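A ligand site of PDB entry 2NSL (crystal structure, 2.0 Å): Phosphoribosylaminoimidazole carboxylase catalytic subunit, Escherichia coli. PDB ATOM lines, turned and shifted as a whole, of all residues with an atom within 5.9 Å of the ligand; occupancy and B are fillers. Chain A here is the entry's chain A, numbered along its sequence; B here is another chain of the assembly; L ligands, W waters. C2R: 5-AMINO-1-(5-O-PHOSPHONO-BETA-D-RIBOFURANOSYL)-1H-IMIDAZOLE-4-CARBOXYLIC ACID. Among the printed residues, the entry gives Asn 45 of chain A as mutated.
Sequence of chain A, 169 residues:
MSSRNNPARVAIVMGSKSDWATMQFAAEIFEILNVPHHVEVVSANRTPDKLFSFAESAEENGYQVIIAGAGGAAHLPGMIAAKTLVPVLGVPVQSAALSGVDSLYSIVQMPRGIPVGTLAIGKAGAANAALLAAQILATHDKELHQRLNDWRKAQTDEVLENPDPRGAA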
ATOM      1  N   MET A  14     -15.042 -11.169 -19.437  1.00  0.00           N
ATOM      2  CA  MET A  14     -15.092 -10.240 -18.309  1.00  0.00           C
ATOM      3  C   MET A  14     -16.527 -10.045 -17.861  1.00  0.00           C
ATOM      4  O   MET A  14     -17.458 -10.178 -18.654  1.00  0.00           O
ATOM      5  CB  MET A  14     -14.470  -8.900 -18.712  1.00  0.00           C
ATOM      6  CG  MET A  14     -15.166  -8.233 -19.889  1.00  0.00           C
ATOM      7  SD  MET A  14     -14.064  -7.211 -20.884  1.00  0.00           S
ATOM      8  CE  MET A  14     -13.306  -8.463 -21.894  1.00  0.00           C
ATOM      9  N   GLY A  15     -16.698  -9.722 -16.576  1.00  0.00           N
ATOM     10  CA  GLY A  15     -18.037  -9.529 -16.031  1.00  0.00           C
ATOM     11  C   GLY A  15     -18.832  -8.353 -16.560  1.00  0.00           C
ATOM     12  O   GLY A  15     -20.061  -8.411 -16.579  1.00  0.00           O
ATOM     13  N   SER A  16     -18.140  -7.294 -16.989  1.00  0.00           N
ATOM     14  CA  SER A  16     -18.827  -6.109 -17.491  1.00  0.00           C
ATOM     15  C   SER A  16     -18.016  -5.383 -18.559  1.00  0.00           C
ATOM     16  O   SER A  16     -16.790  -5.512 -18.615  1.00  0.00           O
ATOM     17  CB  SER A  16     -19.099  -5.136 -16.339  1.00  0.00           C
ATOM     18  OG  SER A  16     -19.738  -3.956 -16.790  1.00  0.00           O
ATOM     19  N   LYS A  17     -18.701  -4.613 -19.394  1.00  0.00           N
ATOM     20  CA  LYS A  17     -18.008  -3.861 -20.428  1.00  0.00           C
ATOM     21  C   LYS A  17     -17.111  -2.822 -19.759  1.00  0.00           C
ATOM     22  O   LYS A  17     -16.132  -2.372 -20.342  1.00  0.00           O
ATOM     23  CB  LYS A  17     -19.019  -3.172 -21.366  1.00  0.00           C
ATOM     24  CG  LYS A  17     -19.961  -2.202 -20.687  1.00  0.00           C
ATOM     25  CD  LYS A  17     -20.935  -1.577 -21.696  1.00  0.00           C
ATOM     26  CE  LYS A  17     -21.873  -0.567 -21.033  1.00  0.00           C
ATOM     27  NZ  LYS A  17     -22.811   0.066 -22.004  1.00  0.00           N
ATOM     28  N   SER A  18     -17.437  -2.463 -18.519  1.00  0.00           N
ATOM     29  CA  SER A  18     -16.634  -1.491 -17.791  1.00  0.00           C
ATOM     30  C   SER A  18     -15.275  -2.098 -17.420  1.00  0.00           C
ATOM     31  O   SER A  18     -14.366  -1.396 -16.987  1.00  0.00           O
ATOM     32  CB  SER A  18     -17.362  -0.988 -16.536  1.00  0.00           C
ATOM     33  OG  SER A  18     -17.669  -2.044 -15.640  1.00  0.00           O
ATOM     34  N   ASP A  19     -15.141  -3.412 -17.602  1.00  0.00           N
ATOM     35  CA  ASP A  19     -13.885  -4.101 -17.302  1.00  0.00           C
ATOM     36  C   ASP A  19     -12.933  -3.980 -18.480  1.00  0.00           C
ATOM     37  O   ASP A  19     -11.718  -4.188 -18.325  1.00  0.00           O
ATOM     38  CB  ASP A  19     -14.116  -5.593 -17.038  1.00  0.00           C
ATOM     39  CG  ASP A  19     -14.858  -5.857 -15.749  1.00  0.00           C
ATOM     40  OD1 ASP A  19     -14.608  -5.148 -14.752  1.00  0.00           O
ATOM     41  OD2 ASP A  19     -15.687  -6.788 -15.737  1.00  0.00           O
ATOM     42  N   VAL A  42     -19.049 -11.842 -20.293  1.00  0.00           N
ATOM     43  CA  VAL A  42     -19.795 -12.946 -19.701  1.00  0.00           C
ATOM     44  C   VAL A  42     -19.867 -12.681 -18.213  1.00  0.00           C
ATOM     45  O   VAL A  42     -18.845 -12.552 -17.551  1.00  0.00           O
ATOM     46  CB  VAL A  42     -19.081 -14.301 -19.942  1.00  0.00           C
ATOM     47  CG1 VAL A  42     -19.878 -15.429 -19.290  1.00  0.00           C
ATOM     48  CG2 VAL A  42     -18.950 -14.549 -21.432  1.00  0.00           C
ATOM     49  N   SER A  43     -21.087 -12.588 -17.683  1.00  0.00           N
ATOM     50  CA  SER A  43     -21.267 -12.319 -16.270  1.00  0.00           C
ATOM     51  C   SER A  43     -21.924 -13.467 -15.537  1.00  0.00           C
ATOM     52  O   SER A  43     -22.962 -13.955 -15.953  1.00  0.00           O
ATOM     53  CB  SER A  43     -22.106 -11.054 -16.061  1.00  0.00           C
ATOM     54  OG  SER A  43     -22.373 -10.860 -14.683  1.00  0.00           O
ATOM     55  N   ALA A  44     -21.308 -13.871 -14.435  1.00  0.00           N
ATOM     56  CA  ALA A  44     -21.836 -14.962 -13.631  1.00  0.00           C
ATOM     57  C   ALA A  44     -23.068 -14.454 -12.911  1.00  0.00           C
ATOM     58  O   ALA A  44     -23.983 -15.223 -12.632  1.00  0.00           O
ATOM     59  CB  ALA A  44     -20.789 -15.415 -12.624  1.00  0.00           C
ATOM     60  N   ASN A  45     -23.104 -13.156 -12.634  1.00  0.00           N
ATOM     61  CA  ASN A  45     -24.216 -12.575 -11.921  1.00  0.00           C
ATOM     62  C   ASN A  45     -25.365 -12.105 -12.808  1.00  0.00           C
ATOM     63  O   ASN A  45     -26.533 -12.211 -12.409  1.00  0.00           O
ATOM     64  CB  ASN A  45     -23.741 -11.396 -11.059  1.00  0.00           C
ATOM     65  CG  ASN A  45     -22.741 -11.835  -9.995  1.00  0.00           C
ATOM     66  OD1 ASN A  45     -22.985 -12.782  -9.246  1.00  0.00           O
ATOM     67  ND2 ASN A  45     -21.627 -11.126  -9.910  1.00  0.00           N
ATOM     68  N   ARG A  46     -25.057 -11.606 -13.993  1.00  0.00           N
ATOM     69  CA  ARG A  46     -26.089 -11.098 -14.899  1.00  0.00           C
ATOM     70  C   ARG A  46     -26.463 -12.035 -16.053  1.00  0.00           C
ATOM     71  O   ARG A  46     -27.572 -11.940 -16.596  1.00  0.00           O
ATOM     72  CB  ARG A  46     -25.653  -9.743 -15.450  1.00  0.00           C
ATOM     73  CG  ARG A  46     -25.548  -8.686 -14.378  1.00  0.00           C
ATOM     74  CD  ARG A  46     -24.725  -7.493 -14.820  1.00  0.00           C
ATOM     75  NE  ARG A  46     -24.694  -6.467 -13.776  1.00  0.00           N
ATOM     76  CZ  ARG A  46     -23.764  -5.515 -13.695  1.00  0.00           C
ATOM     77  NH1 ARG A  46     -22.778  -5.468 -14.581  1.00  0.00           N
ATOM     78  NH2 ARG A  46     -23.839  -4.613 -12.730  1.00  0.00           N
ATOM     79  N   LEU A  51     -23.018 -18.127 -18.970  1.00  0.00           N
ATOM     80  CA  LEU A  51     -21.727 -18.513 -18.437  1.00  0.00           C
ATOM     81  C   LEU A  51     -21.615 -20.040 -18.512  1.00  0.00           C
ATOM     82  O   LEU A  51     -20.619 -20.579 -18.975  1.00  0.00           O
ATOM     83  CB  LEU A  51     -21.577 -18.053 -16.977  1.00  0.00           C
ATOM     84  CG  LEU A  51     -20.209 -18.290 -16.313  1.00  0.00           C
ATOM     85  CD1 LEU A  51     -20.108 -17.458 -15.056  1.00  0.00           C
ATOM     86  CD2 LEU A  51     -20.010 -19.763 -15.992  1.00  0.00           C
ATOM     87  N   GLY A  69     -11.777 -11.801 -16.307  1.00  0.00           N
ATOM     88  CA  GLY A  69     -11.560 -10.680 -15.414  1.00  0.00           C
ATOM     89  C   GLY A  69     -12.848 -10.162 -14.788  1.00  0.00           C
ATOM     90  O   GLY A  69     -13.894 -10.153 -15.432  1.00  0.00           O
ATOM     91  N   ALA A  70     -12.770  -9.733 -13.536  1.00  0.00           N
ATOM     92  CA  ALA A  70     -13.934  -9.203 -12.831  1.00  0.00           C
ATOM     93  C   ALA A  70     -13.520  -8.406 -11.601  1.00  0.00           C
ATOM     94  O   ALA A  70     -12.442  -8.631 -11.041  1.00  0.00           O
ATOM     95  CB  ALA A  70     -14.864 -10.346 -12.423  1.00  0.00           C
ATOM     96  N   GLY A  71     -14.376  -7.483 -11.174  1.00  0.00           N
ATOM     97  CA  GLY A  71     -14.074  -6.670 -10.004  1.00  0.00           C
ATOM     98  C   GLY A  71     -15.071  -6.914  -8.895  1.00  0.00           C
ATOM     99  O   GLY A  71     -16.181  -7.406  -9.144  1.00  0.00           O
ATOM    100  N   GLY A  72     -14.685  -6.556  -7.667  1.00  0.00           N
ATOM    101  CA  GLY A  72     -15.561  -6.754  -6.518  1.00  0.00           C
ATOM    102  C   GLY A  72     -15.639  -8.223  -6.165  1.00  0.00           C
ATOM    103  O   GLY A  72     -14.625  -8.924  -6.171  1.00  0.00           O
ATOM    104  N   ALA A  73     -16.832  -8.695  -5.823  1.00  0.00           N
ATOM    105  CA  ALA A  73     -17.020 -10.108  -5.497  1.00  0.00           C
ATOM    106  C   ALA A  73     -17.011 -10.828  -6.855  1.00  0.00           C
ATOM    107  O   ALA A  73     -18.060 -11.063  -7.453  1.00  0.00           O
ATOM    108  CB  ALA A  73     -18.365 -10.305  -4.796  1.00  0.00           C
ATOM    109  N   ALA A  74     -15.816 -11.157  -7.325  1.00  0.00           N
ATOM    110  CA  ALA A  74     -15.648 -11.820  -8.619  1.00  0.00           C
ATOM    111  C   ALA A  74     -15.978 -13.303  -8.572  1.00  0.00           C
ATOM    112  O   ALA A  74     -15.298 -14.096  -7.912  1.00  0.00           O
ATOM    113  CB  ALA A  74     -14.217 -11.611  -9.121  1.00  0.00           C
ATOM    114  N   HIS A  75     -17.026 -13.684  -9.275  1.00  0.00           N
ATOM    115  CA  HIS A  75     -17.459 -15.066  -9.313  1.00  0.00           C
ATOM    116  C   HIS A  75     -17.214 -15.677 -10.682  1.00  0.00           C
ATOM    117  O   HIS A  75     -17.149 -16.899 -10.834  1.00  0.00           O
ATOM    118  CB  HIS A  75     -18.944 -15.136  -8.966  1.00  0.00           C
ATOM    119  CG  HIS A  75     -19.256 -14.676  -7.584  1.00  0.00           C
ATOM    120  ND1 HIS A  75     -20.524 -14.315  -7.177  1.00  0.00           N
ATOM    121  CD2 HIS A  75     -18.468 -14.533  -6.495  1.00  0.00           C
ATOM    122  CE1 HIS A  75     -20.505 -13.964  -5.902  1.00  0.00           C
ATOM    123  NE2 HIS A  75     -19.263 -14.087  -5.464  1.00  0.00           N
ATOM    124  N   LEU A  76     -17.079 -14.819 -11.691  1.00  0.00           N
ATOM    125  CA  LEU A  76     -16.862 -15.270 -13.047  1.00  0.00           C
ATOM    126  C   LEU A  76     -15.749 -16.299 -13.242  1.00  0.00           C
ATOM    127  O   LEU A  76     -16.007 -17.409 -13.707  1.00  0.00           O
ATOM    128  CB  LEU A  76     -16.622 -14.057 -13.962  1.00  0.00           C
ATOM    129  CG  LEU A  76     -16.271 -14.355 -15.421  1.00  0.00           C
ATOM    130  CD1 LEU A  76     -17.393 -15.135 -16.116  1.00  0.00           C
ATOM    131  CD2 LEU A  76     -16.012 -13.036 -16.120  1.00  0.00           C
ATOM    132  N   PRO A  77     -14.498 -15.971 -12.865  1.00  0.00           N
ATOM    133  CA  PRO A  77     -13.401 -16.919 -13.035  1.00  0.00           C
ATOM    134  C   PRO A  77     -13.657 -18.287 -12.413  1.00  0.00           C
ATOM    135  O   PRO A  77     -13.507 -19.330 -13.066  1.00  0.00           O
ATOM    136  CB  PRO A  77     -12.214 -16.212 -12.362  1.00  0.00           C
ATOM    137  CG  PRO A  77     -12.551 -14.773 -12.493  1.00  0.00           C
ATOM    138  CD  PRO A  77     -14.029 -14.758 -12.170  1.00  0.00           C
ATOM    139  N   VAL A  93      -9.915  -7.051 -11.343  1.00  0.00           N
ATOM    140  CA  VAL A  93     -10.086  -5.683 -11.819  1.00  0.00           C
ATOM    141  C   VAL A  93     -10.067  -4.775 -10.599  1.00  0.00           C
ATOM    142  O   VAL A  93     -10.626  -5.120  -9.555  1.00  0.00           O
ATOM    143  CB  VAL A  93     -11.427  -5.518 -12.563  1.00  0.00           C
ATOM    144  CG1 VAL A  93     -11.648  -4.061 -12.965  1.00  0.00           C
ATOM    145  CG2 VAL A  93     -11.438  -6.411 -13.781  1.00  0.00           C
ATOM    146  N   PRO B 111     -22.079  -6.698  -7.238  1.00  0.00           N
ATOM    147  CA  PRO B 111     -22.313  -5.535  -8.080  1.00  0.00           C
ATOM    148  C   PRO B 111     -23.796  -5.210  -8.159  1.00  0.00           C
ATOM    149  O   PRO B 111     -24.639  -6.024  -7.768  1.00  0.00           O
ATOM    150  CB  PRO B 111     -21.752  -5.976  -9.427  1.00  0.00           C
ATOM    151  CG  PRO B 111     -22.156  -7.411  -9.470  1.00  0.00           C
ATOM    152  CD  PRO B 111     -21.840  -7.905  -8.065  1.00  0.00           C
ATOM    153  N   ARG B 112     -24.126  -4.027  -8.667  1.00  0.00           N
ATOM    154  CA  ARG B 112     -25.514  -3.594  -8.784  1.00  0.00           C
ATOM    155  C   ARG B 112     -26.362  -4.561  -9.613  1.00  0.00           C
ATOM    156  O   ARG B 112     -25.993  -4.921 -10.730  1.00  0.00           O
ATOM    157  CB  ARG B 112     -25.556  -2.198  -9.423  1.00  0.00           C
ATOM    158  CG  ARG B 112     -26.953  -1.653  -9.690  1.00  0.00           C
ATOM    159  CD  ARG B 112     -26.869  -0.167 -10.004  1.00  0.00           C
ATOM    160  NE  ARG B 112     -28.184   0.460 -10.179  1.00  0.00           N
ATOM    161  CZ  ARG B 112     -28.942   0.314 -11.259  1.00  0.00           C
ATOM    162  NH1 ARG B 112     -28.532  -0.450 -12.263  1.00  0.00           N
ATOM    163  NH2 ARG B 112     -30.118   0.924 -11.330  1.00  0.00           N
HETATM  164  PA  C2R L   1     -20.766  -2.562 -13.588  1.00  0.00           P
HETATM  165  O1A C2R L   1     -21.406  -3.184 -14.919  1.00  0.00           O
HETATM  166  O2A C2R L   1     -19.893  -1.291 -14.067  1.00  0.00           O
HETATM  167  O3A C2R L   1     -21.778  -2.211 -12.565  1.00  0.00           O
HETATM  168  O5' C2R L   1     -19.711  -3.656 -13.058  1.00  0.00           O
HETATM  169  C2' C2R L   1     -17.655  -6.415 -13.061  1.00  0.00           C
HETATM  170  O2' C2R L   1     -16.537  -7.226 -13.434  1.00  0.00           O
HETATM  171  C3' C2R L   1     -17.187  -5.031 -12.636  1.00  0.00           C
HETATM  172  O3' C2R L   1     -15.857  -5.095 -12.137  1.00  0.00           O
HETATM  173  C5' C2R L   1     -18.974  -3.434 -11.861  1.00  0.00           C
HETATM  174  C4' C2R L   1     -18.155  -4.679 -11.504  1.00  0.00           C
HETATM  175  O4' C2R L   1     -19.030  -5.807 -11.363  1.00  0.00           O
HETATM  176  C1' C2R L   1     -18.199  -6.910 -11.722  1.00  0.00           C
HETATM  177  N1  C2R L   1     -18.945  -8.172 -11.951  1.00  0.00           N
HETATM  178  C5  C2R L   1     -18.668  -9.356 -11.402  1.00  0.00           C
HETATM  179  C4  C2R L   1     -19.496 -10.291 -11.998  1.00  0.00           C
HETATM  180  N3  C2R L   1     -20.270  -9.648 -12.867  1.00  0.00           N
HETATM  181  C2  C2R L   1     -19.932  -8.362 -12.826  1.00  0.00           C
HETATM  182  N5  C2R L   1     -17.801  -9.578 -10.416  1.00  0.00           N
HETATM  183  C6  C2R L   1     -19.448 -11.802 -11.767  1.00  0.00           C
HETATM  184  O7  C2R L   1     -18.701 -12.236 -10.871  1.00  0.00           O
HETATM  185  O8  C2R L   1     -20.150 -12.521 -12.514  1.00  0.00           O
HETATM  186  O   HOH W   1     -15.241  -3.024 -10.337  1.00  0.00           O
HETATM  187  O   HOH W   2     -15.307  -2.592 -14.138  1.00  0.00           O
HETATM  188  O   HOH W   3     -22.028  -2.281  -9.686  1.00  0.00           O
HETATM  189  O   HOH W   4     -18.172  -0.100 -12.270  1.00  0.00           O
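Water W3 bridges O3A of the ligand (2.9 Å) and N of Arg 112 of chain B (2.9 Å).
Water W2 lies within hydrogen-bond range of OD1 of Asp 19 (2.7 Å), OG of Ser 18 (2.9 Å) and O3' of the ligand (3.3 Å).
N of Val 93 is in hydrogen-bond range of O of Ala 70, at 3.0 Å.
The side-chain carboxylate (OD2) of Asp 19 lies within hydrogen-bond range of the backbone NH (N) of Ser 16, at 2.8 Å.
The backbone NH (N) of Asn 45 lies close to the side-chain hydroxyl (OG) of Ser 43, 3.2 Å away.
The backbone NH of Arg 46 lies within hydrogen-bond range of the side-chain hydroxyl of Ser 43, 2.9 Å away.
The guanidinium group (NH2) of Arg 46 lies within hydrogen-bond range of the backbone carbonyl oxygen (O) of Arg 112 of chain B (3.0 Å).
N of Gly 15 lies within hydrogen-bond range of O of Gly 69, 3.1 Å away.
The backbone NH of Gly 15 is in hydrogen-bond range of the side-chain carboxylate of Asp 19 (3.2 Å).
OG of Ser 18 is in hydrogen-bond range of OG of Ser 16.
The backbone NH (N) of Ala 44 sits at hydrogen-bond distance from an oxygen (O8) of the ligand (2.6 Å).
O3' of the ligand sits at hydrogen-bond distance from N of Gly 71 (3.0 Å).
O1A of the ligand lies within salt-bridge range of NH1 of Arg 46 (2.7 Å).
N of Leu 76 sits at hydrogen-bond distance from O7 of the ligand (3.2 Å).
The side-chain hydroxyl of Ser 16 sits at hydrogen-bond distance from an oxygen (O1A) of the ligand (2.6 Å).
The side-chain carboxylate (OD2) of Asp 19 lies within hydrogen-bond range of an oxygen (O2') of the ligand (2.5 Å).
O of Ala 73 sits at hydrogen-bond distance from N5 of the ligand (3.3 Å).
O8 of the ligand sits at hydrogen-bond distance from N of Asn 45 (3.0 Å).
A nitrogen (N5) of the ligand lies within hydrogen-bond range of the backbone carbonyl oxygen of Gly 71 (3.0 Å).
An oxygen (O7) of the ligand lies close to the side-chain amide nitrogen (ND2) of Asn 45 (3.3 Å).
The backbone NH (N) of His 75 is in hydrogen-bond range of an oxygen (O7) of the ligand, 2.7 Å away.
OG of Ser 43 is in hydrogen-bond range of N3 of the ligand, 3.0 Å away.
The side-chain hydroxyl of Ser 18 lies within hydrogen-bond range of an oxygen (O2A) of the ligand, at 2.8 Å.
Merely in contact with the ligand: Gly 15 (3.8 Å), Ala 70 (3.3 Å), Ala 74 (3.6 Å) and Pro 111 of chain B (3.3 Å).
Of the 24 residues printed, 15 come within 4 Å of the ligand.
The nearest printed residue that does not touch the ligand is Val 93 (4.4 Å).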
